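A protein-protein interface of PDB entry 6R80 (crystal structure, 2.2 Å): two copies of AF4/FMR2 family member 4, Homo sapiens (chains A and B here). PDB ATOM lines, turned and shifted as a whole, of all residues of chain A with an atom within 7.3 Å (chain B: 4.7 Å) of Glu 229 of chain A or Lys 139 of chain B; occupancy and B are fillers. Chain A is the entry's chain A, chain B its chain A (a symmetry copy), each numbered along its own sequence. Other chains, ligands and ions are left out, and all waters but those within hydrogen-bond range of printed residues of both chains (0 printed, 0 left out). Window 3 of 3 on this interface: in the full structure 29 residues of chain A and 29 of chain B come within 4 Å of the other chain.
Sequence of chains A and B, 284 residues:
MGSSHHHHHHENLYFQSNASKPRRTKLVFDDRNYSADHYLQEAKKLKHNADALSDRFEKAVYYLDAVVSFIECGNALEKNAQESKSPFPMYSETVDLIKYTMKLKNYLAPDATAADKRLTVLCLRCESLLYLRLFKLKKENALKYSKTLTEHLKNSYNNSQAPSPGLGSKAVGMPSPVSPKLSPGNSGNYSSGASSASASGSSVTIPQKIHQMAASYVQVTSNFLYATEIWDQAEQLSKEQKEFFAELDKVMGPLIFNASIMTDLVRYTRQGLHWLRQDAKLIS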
ATOM      1  N   LEU A 124      31.844 -12.283   4.042  1.00  0.00           N
ATOM      2  CA  LEU A 124      31.207 -12.861   2.862  1.00  0.00           C
ATOM      3  C   LEU A 124      32.076 -13.942   2.236  1.00  0.00           C
ATOM      4  O   LEU A 124      31.555 -14.944   1.737  1.00  0.00           O
ATOM      5  CB  LEU A 124      30.890 -11.766   1.843  1.00  0.00           C
ATOM      6  CG  LEU A 124      29.813 -10.758   2.245  1.00  0.00           C
ATOM      7  CD1 LEU A 124      29.820  -9.579   1.289  1.00  0.00           C
ATOM      8  CD2 LEU A 124      28.428 -11.398   2.287  1.00  0.00           C
ATOM      9  N   SER A 128      30.575 -17.631   1.911  1.00  0.00           N
ATOM     10  CA  SER A 128      30.493 -18.238   0.588  1.00  0.00           C
ATOM     11  C   SER A 128      31.206 -19.584   0.551  1.00  0.00           C
ATOM     12  O   SER A 128      30.615 -20.606   0.188  1.00  0.00           O
ATOM     13  CB  SER A 128      31.081 -17.284  -0.451  1.00  0.00           C
ATOM     14  OG  SER A 128      31.237 -17.930  -1.697  1.00  0.00           O
ATOM     15  N   ASN A 223      22.696 -24.877  -0.924  1.00  0.00           N
ATOM     16  CA  ASN A 223      23.987 -24.486  -0.357  1.00  0.00           C
ATOM     17  C   ASN A 223      24.938 -23.966  -1.424  1.00  0.00           C
ATOM     18  O   ASN A 223      25.662 -22.989  -1.196  1.00  0.00           O
ATOM     19  CB  ASN A 223      24.620 -25.669   0.380  1.00  0.00           C
ATOM     20  CG  ASN A 223      23.961 -25.947   1.715  1.00  0.00           C
ATOM     21  OD1 ASN A 223      23.540 -25.027   2.416  1.00  0.00           O
ATOM     22  ND2 ASN A 223      23.865 -27.223   2.074  1.00  0.00           N
ATOM     23  N   PHE A 224      24.954 -24.588  -2.604  1.00  0.00           N
ATOM     24  CA  PHE A 224      25.792 -24.026  -3.652  1.00  0.00           C
ATOM     25  C   PHE A 224      25.214 -22.722  -4.183  1.00  0.00           C
ATOM     26  O   PHE A 224      25.963 -21.780  -4.466  1.00  0.00           O
ATOM     27  CB  PHE A 224      25.998 -24.976  -4.823  1.00  0.00           C
ATOM     28  CG  PHE A 224      26.747 -24.322  -5.938  1.00  0.00           C
ATOM     29  CD1 PHE A 224      28.058 -23.926  -5.733  1.00  0.00           C
ATOM     30  CD2 PHE A 224      26.127 -23.993  -7.133  1.00  0.00           C
ATOM     31  CE1 PHE A 224      28.764 -23.273  -6.715  1.00  0.00           C
ATOM     32  CE2 PHE A 224      26.834 -23.344  -8.132  1.00  0.00           C
ATOM     33  CZ  PHE A 224      28.153 -22.984  -7.918  1.00  0.00           C
ATOM     34  N   LEU A 225      23.892 -22.658  -4.361  1.00  0.00           N
ATOM     35  CA  LEU A 225      23.281 -21.437  -4.872  1.00  0.00           C
ATOM     36  C   LEU A 225      23.644 -20.246  -3.998  1.00  0.00           C
ATOM     37  O   LEU A 225      23.923 -19.156  -4.506  1.00  0.00           O
ATOM     38  CB  LEU A 225      21.764 -21.600  -4.963  1.00  0.00           C
ATOM     39  CG  LEU A 225      21.233 -22.641  -5.948  1.00  0.00           C
ATOM     40  CD1 LEU A 225      19.728 -22.807  -5.781  1.00  0.00           C
ATOM     41  CD2 LEU A 225      21.576 -22.257  -7.381  1.00  0.00           C
ATOM     42  N   TYR A 226      23.665 -20.445  -2.677  1.00  0.00           N
ATOM     43  CA  TYR A 226      24.079 -19.379  -1.774  1.00  0.00           C
ATOM     44  C   TYR A 226      25.564 -19.074  -1.927  1.00  0.00           C
ATOM     45  O   TYR A 226      25.973 -17.909  -1.867  1.00  0.00           O
ATOM     46  CB  TYR A 226      23.753 -19.757  -0.326  1.00  0.00           C
ATOM     47  CG  TYR A 226      22.296 -20.095  -0.093  1.00  0.00           C
ATOM     48  CD1 TYR A 226      21.303 -19.151  -0.312  1.00  0.00           C
ATOM     49  CD2 TYR A 226      21.915 -21.354   0.355  1.00  0.00           C
ATOM     50  CE1 TYR A 226      19.970 -19.454  -0.105  1.00  0.00           C
ATOM     51  CE2 TYR A 226      20.584 -21.667   0.564  1.00  0.00           C
ATOM     52  CZ  TYR A 226      19.616 -20.712   0.334  1.00  0.00           C
ATOM     53  OH  TYR A 226      18.289 -21.010   0.542  1.00  0.00           O
ATOM     54  N   ALA A 227      26.386 -20.107  -2.131  1.00  0.00           N
ATOM     55  CA  ALA A 227      27.826 -19.905  -2.267  1.00  0.00           C
ATOM     56  C   ALA A 227      28.145 -19.029  -3.472  1.00  0.00           C
ATOM     57  O   ALA A 227      28.976 -18.116  -3.390  1.00  0.00           O
ATOM     58  CB  ALA A 227      28.537 -21.255  -2.380  1.00  0.00           C
ATOM     59  N   THR A 228      27.491 -19.297  -4.606  1.00  0.00           N
ATOM     60  CA  THR A 228      27.706 -18.483  -5.798  1.00  0.00           C
ATOM     61  C   THR A 228      27.256 -17.047  -5.571  1.00  0.00           C
ATOM     62  O   THR A 228      27.986 -16.099  -5.887  1.00  0.00           O
ATOM     63  CB  THR A 228      26.953 -19.083  -6.985  1.00  0.00           C
ATOM     64  OG1 THR A 228      27.242 -20.476  -7.065  1.00  0.00           O
ATOM     65  CG2 THR A 228      27.382 -18.431  -8.277  1.00  0.00           C
ATOM     66  N   GLU A 229      26.055 -16.868  -5.019  1.00  0.00           N
ATOM     67  CA  GLU A 229      25.502 -15.530  -4.849  1.00  0.00           C
ATOM     68  C   GLU A 229      26.311 -14.714  -3.849  1.00  0.00           C
ATOM     69  O   GLU A 229      26.582 -13.532  -4.084  1.00  0.00           O
ATOM     70  CB  GLU A 229      24.040 -15.628  -4.414  1.00  0.00           C
ATOM     71  CG  GLU A 229      23.133 -16.182  -5.494  1.00  0.00           C
ATOM     72  CD  GLU A 229      23.238 -15.388  -6.779  1.00  0.00           C
ATOM     73  OE1 GLU A 229      23.230 -14.142  -6.705  1.00  0.00           O
ATOM     74  OE2 GLU A 229      23.344 -16.008  -7.857  1.00  0.00           O
ATOM     75  N   ILE A 230      26.706 -15.326  -2.732  1.00  0.00           N
ATOM     76  CA  ILE A 230      27.477 -14.592  -1.735  1.00  0.00           C
ATOM     77  C   ILE A 230      28.886 -14.309  -2.248  1.00  0.00           C
ATOM     78  O   ILE A 230      29.483 -13.282  -1.905  1.00  0.00           O
ATOM     79  CB  ILE A 230      27.480 -15.370  -0.402  1.00  0.00           C
ATOM     80  CG1 ILE A 230      26.057 -15.456   0.166  1.00  0.00           C
ATOM     81  CG2 ILE A 230      28.425 -14.732   0.620  1.00  0.00           C
ATOM     82  CD1 ILE A 230      25.882 -16.534   1.205  1.00  0.00           C
ATOM     83  N   TRP A 231      29.431 -15.192  -3.092  1.00  0.00           N
ATOM     84  CA  TRP A 231      30.761 -14.957  -3.652  1.00  0.00           C
ATOM     85  C   TRP A 231      30.756 -13.758  -4.585  1.00  0.00           C
ATOM     86  O   TRP A 231      31.664 -12.919  -4.536  1.00  0.00           O
ATOM     87  CB  TRP A 231      31.253 -16.200  -4.394  1.00  0.00           C
ATOM     88  CG  TRP A 231      32.614 -16.034  -5.000  1.00  0.00           C
ATOM     89  CD1 TRP A 231      32.903 -15.669  -6.284  1.00  0.00           C
ATOM     90  CD2 TRP A 231      33.873 -16.228  -4.346  1.00  0.00           C
ATOM     91  NE1 TRP A 231      34.263 -15.623  -6.468  1.00  0.00           N
ATOM     92  CE2 TRP A 231      34.881 -15.962  -5.295  1.00  0.00           C
ATOM     93  CE3 TRP A 231      34.245 -16.599  -3.051  1.00  0.00           C
ATOM     94  CZ2 TRP A 231      36.239 -16.056  -4.988  1.00  0.00           C
ATOM     95  CZ3 TRP A 231      35.594 -16.692  -2.749  1.00  0.00           C
ATOM     96  CH2 TRP A 231      36.572 -16.422  -3.711  1.00  0.00           C
ATOM     97  N   ASP A 232      29.744 -13.663  -5.450  1.00  0.00           N
ATOM     98  CA  ASP A 232      29.602 -12.492  -6.307  1.00  0.00           C
ATOM     99  C   ASP A 232      29.397 -11.229  -5.481  1.00  0.00           C
ATOM    100  O   ASP A 232      29.906 -10.161  -5.833  1.00  0.00           O
ATOM    101  CB  ASP A 232      28.441 -12.686  -7.285  1.00  0.00           C
ATOM    102  CG  ASP A 232      28.222 -11.474  -8.175  1.00  0.00           C
ATOM    103  OD1 ASP A 232      29.099 -11.186  -9.016  1.00  0.00           O
ATOM    104  OD2 ASP A 232      27.182 -10.798  -8.029  1.00  0.00           O
ATOM    105  N   GLN A 233      28.662 -11.335  -4.372  1.00  0.00           N
ATOM    106  CA  GLN A 233      28.451 -10.185  -3.497  1.00  0.00           C
ATOM    107  C   GLN A 233      29.770  -9.700  -2.901  1.00  0.00           C
ATOM    108  O   GLN A 233      30.054  -8.497  -2.889  1.00  0.00           O
ATOM    109  CB  GLN A 233      27.460 -10.565  -2.398  1.00  0.00           C
ATOM    110  CG  GLN A 233      27.108  -9.454  -1.446  1.00  0.00           C
ATOM    111  CD  GLN A 233      25.983  -9.844  -0.514  1.00  0.00           C
ATOM    112  OE1 GLN A 233      25.236 -10.787  -0.782  1.00  0.00           O
ATOM    113  NE2 GLN A 233      25.859  -9.124   0.589  1.00  0.00           N
ATOM    114  N   ALA A 234      30.585 -10.629  -2.395  1.00  0.00           N
ATOM    115  CA  ALA A 234      31.933 -10.286  -1.950  1.00  0.00           C
ATOM    116  C   ALA A 234      32.761  -9.705  -3.089  1.00  0.00           C
ATOM    117  O   ALA A 234      33.515  -8.747  -2.891  1.00  0.00           O
ATOM    118  CB  ALA A 234      32.618 -11.522  -1.368  1.00  0.00           C
ATOM    119  N   GLU A 235      32.632 -10.271  -4.290  1.00  0.00           N
ATOM    120  CA  GLU A 235      33.404  -9.772  -5.423  1.00  0.00           C
ATOM    121  C   GLU A 235      33.001  -8.345  -5.775  1.00  0.00           C
ATOM    122  O   GLU A 235      33.858  -7.510  -6.085  1.00  0.00           O
ATOM    123  CB  GLU A 235      33.228 -10.697  -6.629  1.00  0.00           C
ATOM    124  CG  GLU A 235      34.398 -10.683  -7.603  1.00  0.00           C
ATOM    125  CD  GLU A 235      35.635 -11.350  -7.034  1.00  0.00           C
ATOM    126  OE1 GLU A 235      35.532 -11.984  -5.963  1.00  0.00           O
ATOM    127  OE2 GLU A 235      36.713 -11.241  -7.657  1.00  0.00           O
ATOM    128  N   PHE A 257      37.409 -19.540  -5.653  1.00  0.00           N
ATOM    129  CA  PHE A 257      36.096 -20.029  -5.237  1.00  0.00           C
ATOM    130  C   PHE A 257      36.077 -21.548  -5.096  1.00  0.00           C
ATOM    131  O   PHE A 257      35.738 -22.080  -4.035  1.00  0.00           O
ATOM    132  CB  PHE A 257      35.032 -19.561  -6.234  1.00  0.00           C
ATOM    133  CG  PHE A 257      33.645 -20.041  -5.914  1.00  0.00           C
ATOM    134  CD1 PHE A 257      32.948 -19.518  -4.838  1.00  0.00           C
ATOM    135  CD2 PHE A 257      33.035 -21.009  -6.696  1.00  0.00           C
ATOM    136  CE1 PHE A 257      31.670 -19.957  -4.541  1.00  0.00           C
ATOM    137  CE2 PHE A 257      31.756 -21.451  -6.405  1.00  0.00           C
ATOM    138  CZ  PHE A 257      31.073 -20.923  -5.325  1.00  0.00           C
ATOM    139  N   PHE B 135      24.246 -23.293 -16.434  1.00  0.00           N
ATOM    140  CA  PHE B 135      23.641 -23.025 -15.135  1.00  0.00           C
ATOM    141  C   PHE B 135      23.448 -21.530 -14.917  1.00  0.00           C
ATOM    142  O   PHE B 135      22.358 -21.080 -14.553  1.00  0.00           O
ATOM    143  CB  PHE B 135      24.503 -23.621 -14.020  1.00  0.00           C
ATOM    144  CG  PHE B 135      24.344 -22.927 -12.696  1.00  0.00           C
ATOM    145  CD1 PHE B 135      23.133 -22.957 -12.020  1.00  0.00           C
ATOM    146  CD2 PHE B 135      25.406 -22.246 -12.124  1.00  0.00           C
ATOM    147  CE1 PHE B 135      22.985 -22.317 -10.803  1.00  0.00           C
ATOM    148  CE2 PHE B 135      25.264 -21.607 -10.905  1.00  0.00           C
ATOM    149  CZ  PHE B 135      24.053 -21.641 -10.245  1.00  0.00           C
ATOM    150  N   LYS B 136      24.502 -20.745 -15.145  1.00  0.00           N
ATOM    151  CA  LYS B 136      24.449 -19.323 -14.819  1.00  0.00           C
ATOM    152  C   LYS B 136      23.401 -18.582 -15.637  1.00  0.00           C
ATOM    153  O   LYS B 136      22.845 -17.585 -15.162  1.00  0.00           O
ATOM    154  CB  LYS B 136      25.824 -18.687 -15.017  1.00  0.00           C
ATOM    155  CG  LYS B 136      26.820 -19.052 -13.934  1.00  0.00           C
ATOM    156  CD  LYS B 136      28.124 -18.305 -14.110  1.00  0.00           C
ATOM    157  CE  LYS B 136      29.105 -18.656 -13.006  1.00  0.00           C
ATOM    158  NZ  LYS B 136      30.393 -17.938 -13.179  1.00  0.00           N
ATOM    159  N   LEU B 137      23.110 -19.048 -16.855  1.00  0.00           N
ATOM    160  CA  LEU B 137      22.125 -18.359 -17.684  1.00  0.00           C
ATOM    161  C   LEU B 137      20.731 -18.418 -17.072  1.00  0.00           C
ATOM    162  O   LEU B 137      19.916 -17.518 -17.300  1.00  0.00           O
ATOM    163  CB  LEU B 137      22.113 -18.955 -19.091  1.00  0.00           C
ATOM    164  CG  LEU B 137      23.350 -18.686 -19.951  1.00  0.00           C
ATOM    165  CD1 LEU B 137      23.249 -19.435 -21.271  1.00  0.00           C
ATOM    166  CD2 LEU B 137      23.522 -17.193 -20.189  1.00  0.00           C
ATOM    167  N   LYS B 138      20.440 -19.459 -16.289  1.00  0.00           N
ATOM    168  CA  LYS B 138      19.128 -19.631 -15.673  1.00  0.00           C
ATOM    169  C   LYS B 138      19.211 -19.721 -14.154  1.00  0.00           C
ATOM    170  O   LYS B 138      18.336 -20.324 -13.525  1.00  0.00           O
ATOM    171  CB  LYS B 138      18.429 -20.870 -16.237  1.00  0.00           C
ATOM    172  CG  LYS B 138      18.265 -20.875 -17.751  1.00  0.00           C
ATOM    173  CD  LYS B 138      17.311 -21.980 -18.195  1.00  0.00           C
ATOM    174  CE  LYS B 138      17.242 -22.092 -19.711  1.00  0.00           C
ATOM    175  NZ  LYS B 138      16.751 -20.842 -20.349  1.00  0.00           N
ATOM    176  N   LYS B 139      20.243 -19.133 -13.545  1.00  0.00           N
ATOM    177  CA  LYS B 139      20.404 -19.233 -12.100  1.00  0.00           C
ATOM    178  C   LYS B 139      19.445 -18.331 -11.337  1.00  0.00           C
ATOM    179  O   LYS B 139      19.235 -18.548 -10.138  1.00  0.00           O
ATOM    180  CB  LYS B 139      21.844 -18.907 -11.701  1.00  0.00           C
ATOM    181  CG  LYS B 139      22.189 -17.432 -11.751  1.00  0.00           C
ATOM    182  CD  LYS B 139      23.461 -17.147 -10.972  1.00  0.00           C
ATOM    183  CE  LYS B 139      23.796 -15.666 -10.975  1.00  0.00           C
ATOM    184  NZ  LYS B 139      24.796 -15.334  -9.921  1.00  0.00           N
ATOM    185  N   GLU B 140      18.864 -17.324 -11.995  1.00  0.00           N
ATOM    186  CA  GLU B 140      17.830 -16.529 -11.342  1.00  0.00           C
ATOM    187  C   GLU B 140      16.591 -17.371 -11.069  1.00  0.00           C
ATOM    188  O   GLU B 140      15.966 -17.242 -10.010  1.00  0.00           O
ATOM    189  CB  GLU B 140      17.473 -15.316 -12.198  1.00  0.00           C
ATOM    190  CG  GLU B 140      16.465 -14.388 -11.548  1.00  0.00           C
ATOM    191  CD  GLU B 140      15.660 -13.600 -12.559  1.00  0.00           C
ATOM    192  OE1 GLU B 140      15.681 -13.963 -13.754  1.00  0.00           O
ATOM    193  OE2 GLU B 140      15.003 -12.617 -12.158  1.00  0.00           O
ATOM    194  N   ASN B 141      16.220 -18.238 -12.014  1.00  0.00           N
ATOM    195  CA  ASN B 141      15.111 -19.157 -11.780  1.00  0.00           C
ATOM    196  C   ASN B 141      15.422 -20.107 -10.632  1.00  0.00           C
ATOM    197  O   ASN B 141      14.532 -20.463  -9.852  1.00  0.00           O
ATOM    198  CB  ASN B 141      14.806 -19.956 -13.048  1.00  0.00           C
ATOM    199  CG  ASN B 141      14.350 -19.087 -14.204  1.00  0.00           C
ATOM    200  OD1 ASN B 141      14.616 -17.887 -14.241  1.00  0.00           O
ATOM    201  ND2 ASN B 141      13.659 -19.698 -15.161  1.00  0.00           N
ATOM    202  N   ALA B 142      16.686 -20.515 -10.505  1.00  0.00           N
ATOM    203  CA  ALA B 142      17.036 -21.583  -9.574  1.00  0.00           C
ATOM    204  C   ALA B 142      16.890 -21.139  -8.125  1.00  0.00           C
ATOM    205  O   ALA B 142      16.441 -21.917  -7.276  1.00  0.00           O
ATOM    206  CB  ALA B 142      18.460 -22.067  -9.846  1.00  0.00           C
ATOM    207  N   LEU B 143      17.263 -19.896  -7.817  1.00  0.00           N
ATOM    208  CA  LEU B 143      17.245 -19.453  -6.426  1.00  0.00           C
ATOM    209  C   LEU B 143      15.826 -19.186  -5.936  1.00  0.00           C
ATOM    210  O   LEU B 143      15.509 -19.463  -4.773  1.00  0.00           O
ATOM    211  CB  LEU B 143      18.117 -18.207  -6.256  1.00  0.00           C
ATOM    212  CG  LEU B 143      18.464 -17.812  -4.820  1.00  0.00           C
ATOM    213  CD1 LEU B 143      18.978 -19.016  -4.047  1.00  0.00           C
ATOM    214  CD2 LEU B 143      19.489 -16.685  -4.792  1.00  0.00           C
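Of chain B, only Lys 139 and Leu 143 come within 4 Å of Glu 229 of chain A. Trp 231 of chain A touches none of the printed residues of chain B. Of the printed residues of chain A, Phe 135 of chain B touches Phe 224 (3.6 Å) and Leu 225 (3.7 Å). Lys 139 of chain B touches one residue of chain A. Printed residues of chain A within 4 Å of Ala 142 of chain B: Leu 225. Of the printed residues of chain A, Leu 143 of chain B touches Leu 225 (3.9 Å) and Glu 229 (3.7 Å).
Phe 135 of chain B touches Phe 224 of chain A. Leu 225 of chain A touches Phe 135 of chain B (CD2 to CE1, 3.7 Å). Ala 142 of chain B touches Leu 225 of chain A (O to CD1, 3.7 Å). CB of Leu 225 of chain A touches CD1 of Leu 143 of chain B, 3.9 Å away. Glu 229 of chain A touches Leu 143 of chain B (CG to CD2, 3.7 Å).
No position is printed for both chains. Of the 6 pairs that touch across the chains among the printed residues, none has its exchanged pair printed and touching as well.
O of Phe 224 of chain A sits close to OG1 of Thr 228 of chain A, at 3.2 Å.
Of the 9 printed residues of chain B, 4 touch a printed residue of chain A. Hydrophobic or aromatic side chains of chain B within 4 Å of the printed part of chain A: Phe 135, Ala 142 and Leu 143. Of the 16 printed residues of chain A, 3 touch a printed residue of chain B. Hydrophobic or aromatic side chains of chain A within 4 Å of the printed part of chain B: Phe 224 and Leu 225. Among the printed residues, 6 pairs touch across the chains.
The side-chain amino group (NZ) of Lys 139 of chain B is in salt-bridge range of the side-chain carboxylate (OE2) of Glu 229 of chain A (2.6 Å).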
